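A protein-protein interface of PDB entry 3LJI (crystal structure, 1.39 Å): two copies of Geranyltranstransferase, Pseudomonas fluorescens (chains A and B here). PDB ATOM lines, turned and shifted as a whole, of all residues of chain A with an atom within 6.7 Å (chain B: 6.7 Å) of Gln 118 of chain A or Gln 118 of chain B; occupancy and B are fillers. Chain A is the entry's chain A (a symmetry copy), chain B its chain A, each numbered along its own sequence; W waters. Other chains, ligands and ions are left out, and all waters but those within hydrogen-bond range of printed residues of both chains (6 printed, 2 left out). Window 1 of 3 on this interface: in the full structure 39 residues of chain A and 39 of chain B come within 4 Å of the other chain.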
ATOM      1  N   MET A  36      11.469   6.565   9.709  1.00  0.00           N
ATOM      2  CA  MET A  36      12.811   6.230   9.195  1.00  0.00           C
ATOM      3  C   MET A  36      12.740   5.418   7.914  1.00  0.00           C
ATOM      4  O   MET A  36      13.438   5.721   6.971  1.00  0.00           O
ATOM      5  CB  MET A  36      13.627   5.475  10.259  1.00  0.00           C
ATOM      6  CG  MET A  36      13.982   6.330  11.469  1.00  0.00           C
ATOM      7  SD  MET A  36      15.295   5.530  12.617  1.00  0.00           S
ATOM      8  CE  MET A  36      14.334   3.944  13.144  1.00  0.00           C
ATOM      9  N   ALA A  72      25.505   1.581   6.105  1.00  0.00           N
ATOM     10  CA  ALA A  72      25.907   2.740   6.906  1.00  0.00           C
ATOM     11  C   ALA A  72      25.927   4.013   6.076  1.00  0.00           C
ATOM     12  O   ALA A  72      25.387   5.062   6.502  1.00  0.00           O
ATOM     13  CB  ALA A  72      27.247   2.499   7.536  1.00  0.00           C
ATOM     14  N   LEU A  75      22.425   5.120   5.130  1.00  0.00           N
ATOM     15  CA  LEU A  75      21.663   5.622   6.274  1.00  0.00           C
ATOM     16  C   LEU A  75      22.118   7.036   6.632  1.00  0.00           C
ATOM     17  O   LEU A  75      21.278   7.893   6.950  1.00  0.00           O
ATOM     18  CB  LEU A  75      21.841   4.668   7.471  1.00  0.00           C
ATOM     19  CG  LEU A  75      21.242   3.286   7.216  1.00  0.00           C
ATOM     20  CD1 LEU A  75      21.753   2.276   8.274  1.00  0.00           C
ATOM     21  CD2 LEU A  75      19.748   3.388   7.304  1.00  0.00           C
ATOM     22  N   ILE A  76      23.430   7.277   6.574  1.00  0.00           N
ATOM     23  CA  ILE A  76      23.938   8.649   6.794  1.00  0.00           C
ATOM     24  C   ILE A  76      23.398   9.584   5.724  1.00  0.00           C
ATOM     25  O   ILE A  76      22.877  10.654   6.035  1.00  0.00           O
ATOM     26  CB  ILE A  76      25.474   8.706   6.787  1.00  0.00           C
ATOM     27  CG1 ILE A  76      26.095   8.010   7.995  1.00  0.00           C
ATOM     28  CG2 ILE A  76      25.982  10.147   6.690  1.00  0.00           C
ATOM     29  CD1 ILE A  76      25.745   8.579   9.383  1.00  0.00           C
ATOM     30  N   TYR A  79      19.679  10.288   6.361  1.00  0.00           N
ATOM     31  CA  TYR A  79      19.444  11.193   7.488  1.00  0.00           C
ATOM     32  C   TYR A  79      19.736  12.635   7.068  1.00  0.00           C
ATOM     33  O   TYR A  79      18.971  13.545   7.398  1.00  0.00           O
ATOM     34  CB  TYR A  79      20.235  10.758   8.747  1.00  0.00           C
ATOM     35  CG  TYR A  79      21.307  11.719   9.224  1.00  0.00           C
ATOM     36  CD1 TYR A  79      20.971  13.004   9.705  1.00  0.00           C
ATOM     37  CD2 TYR A  79      22.665  11.358   9.188  1.00  0.00           C
ATOM     38  CE1 TYR A  79      21.961  13.875  10.108  1.00  0.00           C
ATOM     39  CE2 TYR A  79      23.662  12.239   9.617  1.00  0.00           C
ATOM     40  CZ  TYR A  79      23.294  13.494  10.071  1.00  0.00           C
ATOM     41  OH  TYR A  79      24.219  14.410  10.482  1.00  0.00           O
ATOM     42  N   ALA A 113      13.658  11.124  13.274  1.00  0.00           N
ATOM     43  CA  ALA A 113      13.978  10.107  12.284  1.00  0.00           C
ATOM     44  C   ALA A 113      15.408  10.286  11.792  1.00  0.00           C
ATOM     45  O   ALA A 113      16.155   9.301  11.677  1.00  0.00           O
ATOM     46  CB  ALA A 113      12.988  10.137  11.153  1.00  0.00           C
ATOM     47  N   GLY A 114      15.818  11.503  11.483  1.00  0.00           N
ATOM     48  CA  GLY A 114      17.182  11.755  11.054  1.00  0.00           C
ATOM     49  C   GLY A 114      18.189  11.423  12.151  1.00  0.00           C
ATOM     50  O   GLY A 114      19.223  10.811  11.868  1.00  0.00           O
ATOM     51  N   ASP A 115      17.910  11.816  13.378  1.00  0.00           N
ATOM     52  CA  ASP A 115      18.807  11.524  14.503  1.00  0.00           C
ATOM     53  C   ASP A 115      18.964  10.016  14.700  1.00  0.00           C
ATOM     54  O   ASP A 115      20.096   9.525  14.928  1.00  0.00           O
ATOM     55  CB  ASP A 115      18.284  12.186  15.770  1.00  0.00           C
ATOM     56  CG  ASP A 115      18.452  13.678  15.763  1.00  0.00           C
ATOM     57  OD1 ASP A 115      19.251  14.214  14.975  1.00  0.00           O
ATOM     58  OD2 ASP A 115      17.808  14.306  16.654  1.00  0.00           O
ATOM     59  N   GLY A 116      17.865   9.279  14.599  1.00  0.00           N
ATOM     60  CA  GLY A 116      17.913   7.818  14.786  1.00  0.00           C
ATOM     61  C   GLY A 116      18.605   7.157  13.611  1.00  0.00           C
ATOM     62  O   GLY A 116      19.291   6.165  13.813  1.00  0.00           O
ATOM     63  N   LEU A 117      18.426   7.654  12.389  1.00  0.00           N
ATOM     64  CA  LEU A 117      19.127   7.090  11.254  1.00  0.00           C
ATOM     65  C   LEU A 117      20.634   7.221  11.401  1.00  0.00           C
ATOM     66  O   LEU A 117      21.375   6.318  10.995  1.00  0.00           O
ATOM     67  CB  LEU A 117      18.673   7.730   9.946  1.00  0.00           C
ATOM     68  CG  LEU A 117      17.305   7.296   9.433  1.00  0.00           C
ATOM     69  CD1 LEU A 117      16.786   8.301   8.380  1.00  0.00           C
ATOM     70  CD2 LEU A 117      17.370   5.905   8.855  1.00  0.00           C
ATOM     71  N   GLN A 118      21.135   8.334  11.936  1.00  0.00           N
ATOM     72  CA  GLN A 118      22.585   8.439  12.133  1.00  0.00           C
ATOM     73  C   GLN A 118      23.056   7.365  13.106  1.00  0.00           C
ATOM     74  O   GLN A 118      24.054   6.696  12.818  1.00  0.00           O
ATOM     75  CB  GLN A 118      23.015   9.840  12.598  1.00  0.00           C
ATOM     76  CG  GLN A 118      24.493   9.836  12.946  1.00  0.00           C
ATOM     77  CD  GLN A 118      25.211  11.156  13.191  1.00  0.00           C
ATOM     78  OE1 GLN A 118      26.432  11.127  13.383  1.00  0.00           O
ATOM     79  NE2 GLN A 118      24.501  12.290  13.257  1.00  0.00           N
ATOM     80  N   SER A 119      22.372   7.175  14.225  1.00  0.00           N
ATOM     81  CA  SER A 119      22.753   6.120  15.188  1.00  0.00           C
ATOM     82  C   SER A 119      22.685   4.762  14.522  1.00  0.00           C
ATOM     83  O   SER A 119      23.602   3.936  14.703  1.00  0.00           O
ATOM     84  CB  SER A 119      21.850   6.129  16.419  1.00  0.00           C
ATOM     85  OG  SER A 119      21.902   7.412  17.040  1.00  0.00           O
ATOM     86  N   LEU A 120      21.614   4.490  13.776  1.00  0.00           N
ATOM     87  CA  LEU A 120      21.479   3.199  13.094  1.00  0.00           C
ATOM     88  C   LEU A 120      22.601   2.961  12.115  1.00  0.00           C
ATOM     89  O   LEU A 120      23.012   1.800  11.905  1.00  0.00           O
ATOM     90  CB  LEU A 120      20.163   3.127  12.357  1.00  0.00           C
ATOM     91  CG  LEU A 120      18.924   2.708  13.089  1.00  0.00           C
ATOM     92  CD1 LEU A 120      17.877   2.546  11.984  1.00  0.00           C
ATOM     93  CD2 LEU A 120      19.154   1.346  13.792  1.00  0.00           C
ATOM     94  N   ALA A 121      23.118   4.013  11.481  1.00  0.00           N
ATOM     95  CA  ALA A 121      24.253   3.865  10.557  1.00  0.00           C
ATOM     96  C   ALA A 121      25.464   3.242  11.262  1.00  0.00           C
ATOM     97  O   ALA A 121      26.149   2.331  10.718  1.00  0.00           O
ATOM     98  CB  ALA A 121      24.652   5.208   9.943  1.00  0.00           C
ATOM     99  N   PHE A 122      25.782   3.741  12.448  1.00  0.00           N
ATOM    100  CA  PHE A 122      26.879   3.182  13.230  1.00  0.00           C
ATOM    101  C   PHE A 122      26.573   1.759  13.649  1.00  0.00           C
ATOM    102  O   PHE A 122      27.456   0.885  13.555  1.00  0.00           O
ATOM    103  CB  PHE A 122      27.242   4.088  14.427  1.00  0.00           C
ATOM    104  CG  PHE A 122      27.906   5.359  14.013  1.00  0.00           C
ATOM    105  CD1 PHE A 122      29.261   5.377  13.716  1.00  0.00           C
ATOM    106  CD2 PHE A 122      27.168   6.519  13.865  1.00  0.00           C
ATOM    107  CE1 PHE A 122      29.887   6.520  13.287  1.00  0.00           C
ATOM    108  CE2 PHE A 122      27.788   7.708  13.421  1.00  0.00           C
ATOM    109  CZ  PHE A 122      29.152   7.695  13.119  1.00  0.00           C
ATOM    110  N   SER A 123      25.338   1.474  14.080  1.00  0.00           N
ATOM    111  CA  SER A 123      24.969   0.093  14.440  1.00  0.00           C
ATOM    112  C   SER A 123      25.136  -0.841  13.261  1.00  0.00           C
ATOM    113  O   SER A 123      25.563  -1.988  13.420  1.00  0.00           O
ATOM    114  CB  SER A 123      23.526   0.022  14.934  1.00  0.00           C
ATOM    115  OG  SER A 123      23.366   0.750  16.135  1.00  0.00           O
ATOM    116  N   LEU A 145      33.836   6.682   9.163  1.00  0.00           N
ATOM    117  CA  LEU A 145      32.467   7.141   8.973  1.00  0.00           C
ATOM    118  C   LEU A 145      32.198   8.367   9.828  1.00  0.00           C
ATOM    119  O   LEU A 145      31.618   9.347   9.350  1.00  0.00           O
ATOM    120  CB  LEU A 145      31.432   6.050   9.301  1.00  0.00           C
ATOM    121  CG  LEU A 145      30.007   6.428   8.888  1.00  0.00           C
ATOM    122  CD1 LEU A 145      29.892   6.472   7.355  1.00  0.00           C
ATOM    123  CD2 LEU A 145      28.966   5.487   9.511  1.00  0.00           C
ATOM    124  N   ALA A 146      32.594   8.350  11.095  1.00  0.00           N
ATOM    125  CA  ALA A 146      32.336   9.502  11.965  1.00  0.00           C
ATOM    126  C   ALA A 146      33.046  10.760  11.458  1.00  0.00           C
ATOM    127  O   ALA A 146      32.483  11.860  11.532  1.00  0.00           O
ATOM    128  CB  ALA A 146      32.759   9.184  13.380  1.00  0.00           C
ATOM    129  N   ALA A 149      31.178  11.957   8.173  1.00  0.00           N
ATOM    130  CA  ALA A 149      29.802  12.403   8.401  1.00  0.00           C
ATOM    131  C   ALA A 149      29.749  13.658   9.230  1.00  0.00           C
ATOM    132  O   ALA A 149      28.760  14.399   9.139  1.00  0.00           O
ATOM    133  CB  ALA A 149      29.014  11.321   9.122  1.00  0.00           C
ATOM    134  N   GLY A 150      30.734  13.881  10.084  1.00  0.00           N
ATOM    135  CA  GLY A 150      30.619  14.899  11.125  1.00  0.00           C
ATOM    136  C   GLY A 150      30.988  16.309  10.745  1.00  0.00           C
ATOM    137  O   GLY A 150      30.944  16.674   9.560  1.00  0.00           O
ATOM    138  N   MET A 154      30.714  15.968   6.201  1.00  0.00           N
ATOM    139  CA  MET A 154      29.361  16.266   5.661  1.00  0.00           C
ATOM    140  C   MET A 154      28.644  17.391   6.386  1.00  0.00           C
ATOM    141  O   MET A 154      28.162  18.350   5.738  1.00  0.00           O
ATOM    142  CB  MET A 154      28.481  15.015   5.621  1.00  0.00           C
ATOM    143  CG  MET A 154      27.154  15.244   4.936  1.00  0.00           C
ATOM    144  SD  MET A 154      26.113  13.608   5.168  1.00  0.00           S
ATOM    145  CE  MET A 154      25.689  13.816   7.052  1.00  0.00           C
ATOM    146  N   VAL A 155      28.553  17.310   7.714  1.00  0.00           N
ATOM    147  CA  VAL A 155      27.831  18.347   8.467  1.00  0.00           C
ATOM    148  C   VAL A 155      28.535  19.680   8.317  1.00  0.00           C
ATOM    149  O   VAL A 155      27.875  20.726   8.154  1.00  0.00           O
ATOM    150  CB  VAL A 155      27.643  17.940   9.940  1.00  0.00           C
ATOM    151  CG1 VAL A 155      27.239  19.133  10.786  1.00  0.00           C
ATOM    152  CG2 VAL A 155      26.590  16.823  10.028  1.00  0.00           C
ATOM    153  N   MET B  36      28.562  24.343  18.388  1.00  0.00           N
ATOM    154  CA  MET B  36      28.722  23.104  19.171  1.00  0.00           C
ATOM    155  C   MET B  36      29.310  23.372  20.544  1.00  0.00           C
ATOM    156  O   MET B  36      28.811  22.861  21.523  1.00  0.00           O
ATOM    157  CB  MET B  36      29.593  22.089  18.409  1.00  0.00           C
ATOM    158  CG  MET B  36      28.932  21.554  17.144  1.00  0.00           C
ATOM    159  SD  MET B  36      29.832  20.035  16.392  1.00  0.00           S
ATOM    160  CE  MET B  36      31.540  20.837  15.999  1.00  0.00           C
ATOM    161  N   ALA B  72      31.992  11.010  25.117  1.00  0.00           N
ATOM    162  CA  ALA B  72      30.961  10.510  24.203  1.00  0.00           C
ATOM    163  C   ALA B  72      29.569  10.677  24.788  1.00  0.00           C
ATOM    164  O   ALA B  72      28.642  11.167  24.099  1.00  0.00           O
ATOM    165  CB  ALA B  72      31.221   9.073  23.860  1.00  0.00           C
ATOM    166  N   LEU B  75      28.537  14.324  24.923  1.00  0.00           N
ATOM    167  CA  LEU B  75      28.282  14.888  23.597  1.00  0.00           C
ATOM    168  C   LEU B  75      26.923  14.423  23.078  1.00  0.00           C
ATOM    169  O   LEU B  75      26.185  15.220  22.477  1.00  0.00           O
ATOM    170  CB  LEU B  75      29.411  14.472  22.634  1.00  0.00           C
ATOM    171  CG  LEU B  75      30.765  15.063  23.024  1.00  0.00           C
ATOM    172  CD1 LEU B  75      31.904  14.341  22.261  1.00  0.00           C
ATOM    173  CD2 LEU B  75      30.772  16.520  22.670  1.00  0.00           C
ATOM    174  N   ILE B  76      26.595  13.150  23.311  1.00  0.00           N
ATOM    175  CA  ILE B  76      25.251  12.655  22.942  1.00  0.00           C
ATOM    176  C   ILE B  76      24.185  13.405  23.725  1.00  0.00           C
ATOM    177  O   ILE B  76      23.217  13.896  23.147  1.00  0.00           O
ATOM    178  CB  ILE B  76      25.099  11.147  23.196  1.00  0.00           C
ATOM    179  CG1 ILE B  76      25.948  10.301  22.251  1.00  0.00           C
ATOM    180  CG2 ILE B  76      23.633  10.710  23.122  1.00  0.00           C
ATOM    181  CD1 ILE B  76      25.643  10.419  20.746  1.00  0.00           C
ATOM    182  N   TYR B  79      23.829  16.974  22.358  1.00  0.00           N
ATOM    183  CA  TYR B  79      23.142  17.036  21.066  1.00  0.00           C
ATOM    184  C   TYR B  79      21.635  16.868  21.269  1.00  0.00           C
ATOM    185  O   TYR B  79      20.843  17.592  20.661  1.00  0.00           O
ATOM    186  CB  TYR B  79      23.732  16.022  20.055  1.00  0.00           C
ATOM    187  CG  TYR B  79      22.801  14.914  19.602  1.00  0.00           C
ATOM    188  CD1 TYR B  79      21.638  15.201  18.854  1.00  0.00           C
ATOM    189  CD2 TYR B  79      23.066  13.573  19.929  1.00  0.00           C
ATOM    190  CE1 TYR B  79      20.787  14.183  18.475  1.00  0.00           C
ATOM    191  CE2 TYR B  79      22.209  12.544  19.525  1.00  0.00           C
ATOM    192  CZ  TYR B  79      21.074  12.866  18.803  1.00  0.00           C
ATOM    193  OH  TYR B  79      20.185  11.913  18.398  1.00  0.00           O
ATOM    194  N   ALA B 113      24.539  21.708  14.495  1.00  0.00           N
ATOM    195  CA  ALA B 113      25.353  21.535  15.688  1.00  0.00           C
ATOM    196  C   ALA B 113      25.006  20.220  16.374  1.00  0.00           C
ATOM    197  O   ALA B 113      25.910  19.474  16.784  1.00  0.00           O
ATOM    198  CB  ALA B 113      25.195  22.709  16.614  1.00  0.00           C
ATOM    199  N   GLY B 114      23.732  19.910  16.529  1.00  0.00           N
ATOM    200  CA  GLY B 114      23.328  18.651  17.129  1.00  0.00           C
ATOM    201  C   GLY B 114      23.776  17.457  16.292  1.00  0.00           C
ATOM    202  O   GLY B 114      24.266  16.470  16.848  1.00  0.00           O
ATOM    203  N   ASP B 115      23.613  17.528  14.987  1.00  0.00           N
ATOM    204  CA  ASP B 115      24.033  16.438  14.097  1.00  0.00           C
ATOM    205  C   ASP B 115      25.540  16.201  14.198  1.00  0.00           C
ATOM    206  O   ASP B 115      25.992  15.031  14.253  1.00  0.00           O
ATOM    207  CB  ASP B 115      23.627  16.750  12.664  1.00  0.00           C
ATOM    208  CG  ASP B 115      22.148  16.634  12.436  1.00  0.00           C
ATOM    209  OD1 ASP B 115      21.439  16.004  13.240  1.00  0.00           O
ATOM    210  OD2 ASP B 115      21.719  17.131  11.353  1.00  0.00           O
ATOM    211  N   GLY B 116      26.316  17.276  14.241  1.00  0.00           N
ATOM    212  CA  GLY B 116      27.782  17.150  14.325  1.00  0.00           C
ATOM    213  C   GLY B 116      28.193  16.655  15.697  1.00  0.00           C
ATOM    214  O   GLY B 116      29.160  15.913  15.790  1.00  0.00           O
ATOM    215  N   LEU B 117      27.510  17.062  16.765  1.00  0.00           N
ATOM    216  CA  LEU B 117      27.831  16.554  18.082  1.00  0.00           C
ATOM    217  C   LEU B 117      27.634  15.050  18.170  1.00  0.00           C
ATOM    218  O   LEU B 117      28.407  14.363  18.847  1.00  0.00           O
ATOM    219  CB  LEU B 117      27.010  17.251  19.162  1.00  0.00           C
ATOM    220  CG  LEU B 117      27.435  18.674  19.507  1.00  0.00           C
ATOM    221  CD1 LEU B 117      26.301  19.402  20.264  1.00  0.00           C
ATOM    222  CD2 LEU B 117      28.703  18.667  20.324  1.00  0.00           C
ATOM    223  N   GLN B 118      26.597  14.498  17.540  1.00  0.00           N
ATOM    224  CA  GLN B 118      26.437  13.040  17.573  1.00  0.00           C
ATOM    225  C   GLN B 118      27.628  12.371  16.897  1.00  0.00           C
ATOM    226  O   GLN B 118      28.176  11.418  17.461  1.00  0.00           O
ATOM    227  CB  GLN B 118      25.110  12.579  16.948  1.00  0.00           C
ATOM    228  CG  GLN B 118      25.081  11.064  16.858  1.00  0.00           C
ATOM    229  CD  GLN B 118      23.779  10.357  16.509  1.00  0.00           C
ATOM    230  OE1 GLN B 118      23.764   9.120  16.533  1.00  0.00           O
ATOM    231  NE2 GLN B 118      22.718  11.079  16.127  1.00  0.00           N
ATOM    232  N   SER B 119      28.045  12.841  15.730  1.00  0.00           N
ATOM    233  CA  SER B 119      29.221  12.263  15.046  1.00  0.00           C
ATOM    234  C   SER B 119      30.450  12.404  15.920  1.00  0.00           C
ATOM    235  O   SER B 119      31.236  11.444  16.043  1.00  0.00           O
ATOM    236  CB  SER B 119      29.475  12.935  13.699  1.00  0.00           C
ATOM    237  OG  SER B 119      28.313  12.816  12.880  1.00  0.00           O
ATOM    238  N   LEU B 120      30.659  13.580  16.512  1.00  0.00           N
ATOM    239  CA  LEU B 120      31.822  13.792  17.378  1.00  0.00           C
ATOM    240  C   LEU B 120      31.823  12.853  18.557  1.00  0.00           C
ATOM    241  O   LEU B 120      32.904  12.449  19.034  1.00  0.00           O
ATOM    242  CB  LEU B 120      31.851  15.215  17.884  1.00  0.00           C
ATOM    243  CG  LEU B 120      32.463  16.292  17.040  1.00  0.00           C
ATOM    244  CD1 LEU B 120      32.501  17.510  17.965  1.00  0.00           C
ATOM    245  CD2 LEU B 120      33.906  15.897  16.637  1.00  0.00           C
ATOM    246  N   ALA B 121      30.650  12.490  19.074  1.00  0.00           N
ATOM    247  CA  ALA B 121      30.570  11.530  20.187  1.00  0.00           C
ATOM    248  C   ALA B 121      31.226  10.195  19.816  1.00  0.00           C
ATOM    249  O   ALA B 121      31.989   9.588  20.618  1.00  0.00           O
ATOM    250  CB  ALA B 121      29.121  11.289  20.612  1.00  0.00           C
ATOM    251  N   PHE B 122      30.915   9.689  18.631  1.00  0.00           N
ATOM    252  CA  PHE B 122      31.528   8.455  18.155  1.00  0.00           C
ATOM    253  C   PHE B 122      33.017   8.637  17.947  1.00  0.00           C
ATOM    254  O   PHE B 122      33.807   7.757  18.340  1.00  0.00           O
ATOM    255  CB  PHE B 122      30.815   7.915  16.895  1.00  0.00           C
ATOM    256  CG  PHE B 122      29.454   7.375  17.185  1.00  0.00           C
ATOM    257  CD1 PHE B 122      29.302   6.096  17.697  1.00  0.00           C
ATOM    258  CD2 PHE B 122      28.333   8.165  17.000  1.00  0.00           C
ATOM    259  CE1 PHE B 122      28.067   5.591  18.016  1.00  0.00           C
ATOM    260  CE2 PHE B 122      27.051   7.671  17.326  1.00  0.00           C
ATOM    261  CZ  PHE B 122      26.928   6.381  17.849  1.00  0.00           C
ATOM    262  N   SER B 123      33.446   9.766  17.372  1.00  0.00           N
ATOM    263  CA  SER B 123      34.888  10.023  17.204  1.00  0.00           C
ATOM    264  C   SER B 123      35.599  10.036  18.540  1.00  0.00           C
ATOM    265  O   SER B 123      36.728   9.551  18.659  1.00  0.00           O
ATOM    266  CB  SER B 123      35.130  11.353  16.495  1.00  0.00           C
ATOM    267  OG  SER B 123      34.626  11.322  15.175  1.00  0.00           O
ATOM    268  N   LEU B 145      26.971   2.437  22.651  1.00  0.00           N
ATOM    269  CA  LEU B 145      26.573   3.833  22.525  1.00  0.00           C
ATOM    270  C   LEU B 145      25.526   3.985  21.434  1.00  0.00           C
ATOM    271  O   LEU B 145      24.518   4.672  21.628  1.00  0.00           O
ATOM    272  CB  LEU B 145      27.765   4.758  22.225  1.00  0.00           C
ATOM    273  CG  LEU B 145      27.412   6.245  22.320  1.00  0.00           C
ATOM    274  CD1 LEU B 145      27.118   6.629  23.780  1.00  0.00           C
ATOM    275  CD2 LEU B 145      28.507   7.130  21.707  1.00  0.00           C
ATOM    276  N   ALA B 146      25.731   3.372  20.275  1.00  0.00           N
ATOM    277  CA  ALA B 146      24.760   3.510  19.185  1.00  0.00           C
ATOM    278  C   ALA B 146      23.393   2.940  19.575  1.00  0.00           C
ATOM    279  O   ALA B 146      22.358   3.516  19.214  1.00  0.00           O
ATOM    280  CB  ALA B 146      25.284   2.834  17.940  1.00  0.00           C
ATOM    281  N   ALA B 149      21.779   5.394  22.237  1.00  0.00           N
ATOM    282  CA  ALA B 149      21.464   6.723  21.706  1.00  0.00           C
ATOM    283  C   ALA B 149      20.372   6.669  20.672  1.00  0.00           C
ATOM    284  O   ALA B 149      19.689   7.682  20.464  1.00  0.00           O
ATOM    285  CB  ALA B 149      22.698   7.336  21.065  1.00  0.00           C
ATOM    286  N   GLY B 150      20.234   5.556  19.970  1.00  0.00           N
ATOM    287  CA  GLY B 150      19.416   5.519  18.762  1.00  0.00           C
ATOM    288  C   GLY B 150      17.941   5.267  18.944  1.00  0.00           C
ATOM    289  O   GLY B 150      17.386   5.531  20.022  1.00  0.00           O
ATOM    290  N   MET B 154      17.531   6.325  23.366  1.00  0.00           N
ATOM    291  CA  MET B 154      17.231   7.762  23.611  1.00  0.00           C
ATOM    292  C   MET B 154      16.290   8.376  22.589  1.00  0.00           C
ATOM    293  O   MET B 154      15.267   8.994  22.967  1.00  0.00           O
ATOM    294  CB  MET B 154      18.510   8.595  23.722  1.00  0.00           C
ATOM    295  CG  MET B 154      18.252  10.028  24.123  1.00  0.00           C
ATOM    296  SD  MET B 154      19.964  10.959  24.011  1.00  0.00           S
ATOM    297  CE  MET B 154      20.102  11.051  22.075  1.00  0.00           C
ATOM    298  N   VAL B 155      16.598   8.228  21.300  1.00  0.00           N
ATOM    299  CA  VAL B 155      15.749   8.839  20.265  1.00  0.00           C
ATOM    300  C   VAL B 155      14.369   8.216  20.295  1.00  0.00           C
ATOM    301  O   VAL B 155      13.353   8.927  20.158  1.00  0.00           O
ATOM    302  CB  VAL B 155      16.408   8.752  18.876  1.00  0.00           C
ATOM    303  CG1 VAL B 155      15.402   9.039  17.778  1.00  0.00           C
ATOM    304  CG2 VAL B 155      17.587   9.736  18.811  1.00  0.00           C
HETATM  305  O   HOH W   1      23.025  16.680   8.543  1.00  0.00           O
HETATM  306  O   HOH W   2      26.596  13.360  10.647  1.00  0.00           O
HETATM  307  O   HOH W   3      21.098   9.512  18.821  1.00  0.00           O
HETATM  308  O   HOH W   4      17.699  13.502  19.678  1.00  0.00           O
HETATM  309  O   HOH W   5      21.233   2.386  16.797  1.00  0.00           O
HETATM  310  O   HOH W   6      33.259  13.357  13.887  1.00  0.00           O
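Gln 118 of chain A touches just these residues of chain B: Asp 115, Gln 118 and Ser 119. Of the printed residues of chain B, Phe 122 of chain A touches Phe 122. Printed residues of chain B within 4 Å of Gly 150 of chain A: Ser 119 (3.4 Å). Of chain A, only Asp 115, Gln 118 and Ser 119 come within 4 Å of Gln 118 of chain B. Ala 121 of chain B touches none of the printed residues of chain A. Of the printed residues of chain A, Phe 122 of chain B touches Phe 122 (3.6 Å). The nearest printed residue of chain B that does not touch Val 155 of chain A is Gly 116 of chain B (4.03 Å).
The side-chain hydroxyl (OG) of Ser 119 of chain B sits at hydrogen-bond distance from the backbone carbonyl oxygen (O) of Asp 115 of chain B (3.5 Å). O of Ala 149 of chain B sits at hydrogen-bond distance from N of Val 155 of chain B, at 3.2 Å. O of Gly 150 of chain B sits at hydrogen-bond distance from N of Val 155 of chain B (3.1 Å).
Of the 22 printed residues of chain B, 9 touch a printed residue of chain A. Hydrophobic or aromatic side chains of chain B within 4 Å of the printed part of chain A: Tyr 79, Phe 122, Ala 146 and Val 155.
The side-chain amide nitrogen (NE2) of Gln 118 of chain A is in hydrogen-bond range of the backbone carbonyl oxygen (O) of Asp 115 of chain B (3.3 Å). NE2 of Gln 118 of chain B sits at hydrogen-bond distance from O of Asp 115 of chain A (3.3 Å). The side-chain amide oxygen of Gln 118 of chain B sits at hydrogen-bond distance from the side-chain hydroxyl of Ser 119 of chain A (2.6 Å). The side-chain hydroxyl of Ser 119 of chain B lies within hydrogen-bond range of the side-chain amide oxygen of Gln 118 of chain A (2.6 Å). OD1 of Asp 115 of chain B lies close to OD1 of Asp 115 of chain A, at 3.3 Å.
Asp 115 of chain A touches Gln 118 of chain B, and with the chains exchanged Gln 118 of chain A touches Asp 115 of chain B. Gln 118 of chain A touches Ser 119 of chain B, and with the chains exchanged Ser 119 of chain A touches Gln 118 of chain B. 22 positions are printed for both chains.
Water W2 lies within hydrogen-bond range of OH of Tyr 79 of chain A, O of Ala 149 of chain A and OG of Ser 119 of chain B. Water W6 bridges OG of Ser 123 of chain B (2.8 Å) and O of Ala 146 of chain A (2.9 Å). Water W5 bridges OG of Ser 123 of chain A (2.8 Å) and O of Ala 146 of chain B (2.9 Å).
Among the printed residues, merely in contact across the chains: Tyr 79 of chain A with Asp 115 of chain B, Asp 115 of chain A with Tyr 79 of chain B, Ala 146 of chain A with Ser 123 of chain B, Ser 123 of chain A with Ala 146 of chain B, Ser 119 of chain A with Gly 150 of chain B, Gly 150 of chain A with Ser 119 of chain B, Gln 118 of chain A with Gln 118 of chain B, Phe 122 of chain A with Phe 122 of chain B, Ala 146 of chain A with Ser 119 of chain B, Ser 119 of chain A with Ala 146 of chain B, Val 155 of chain A with Asp 115 of chain B and Asp 115 of chain A with Val 155 of chain B.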
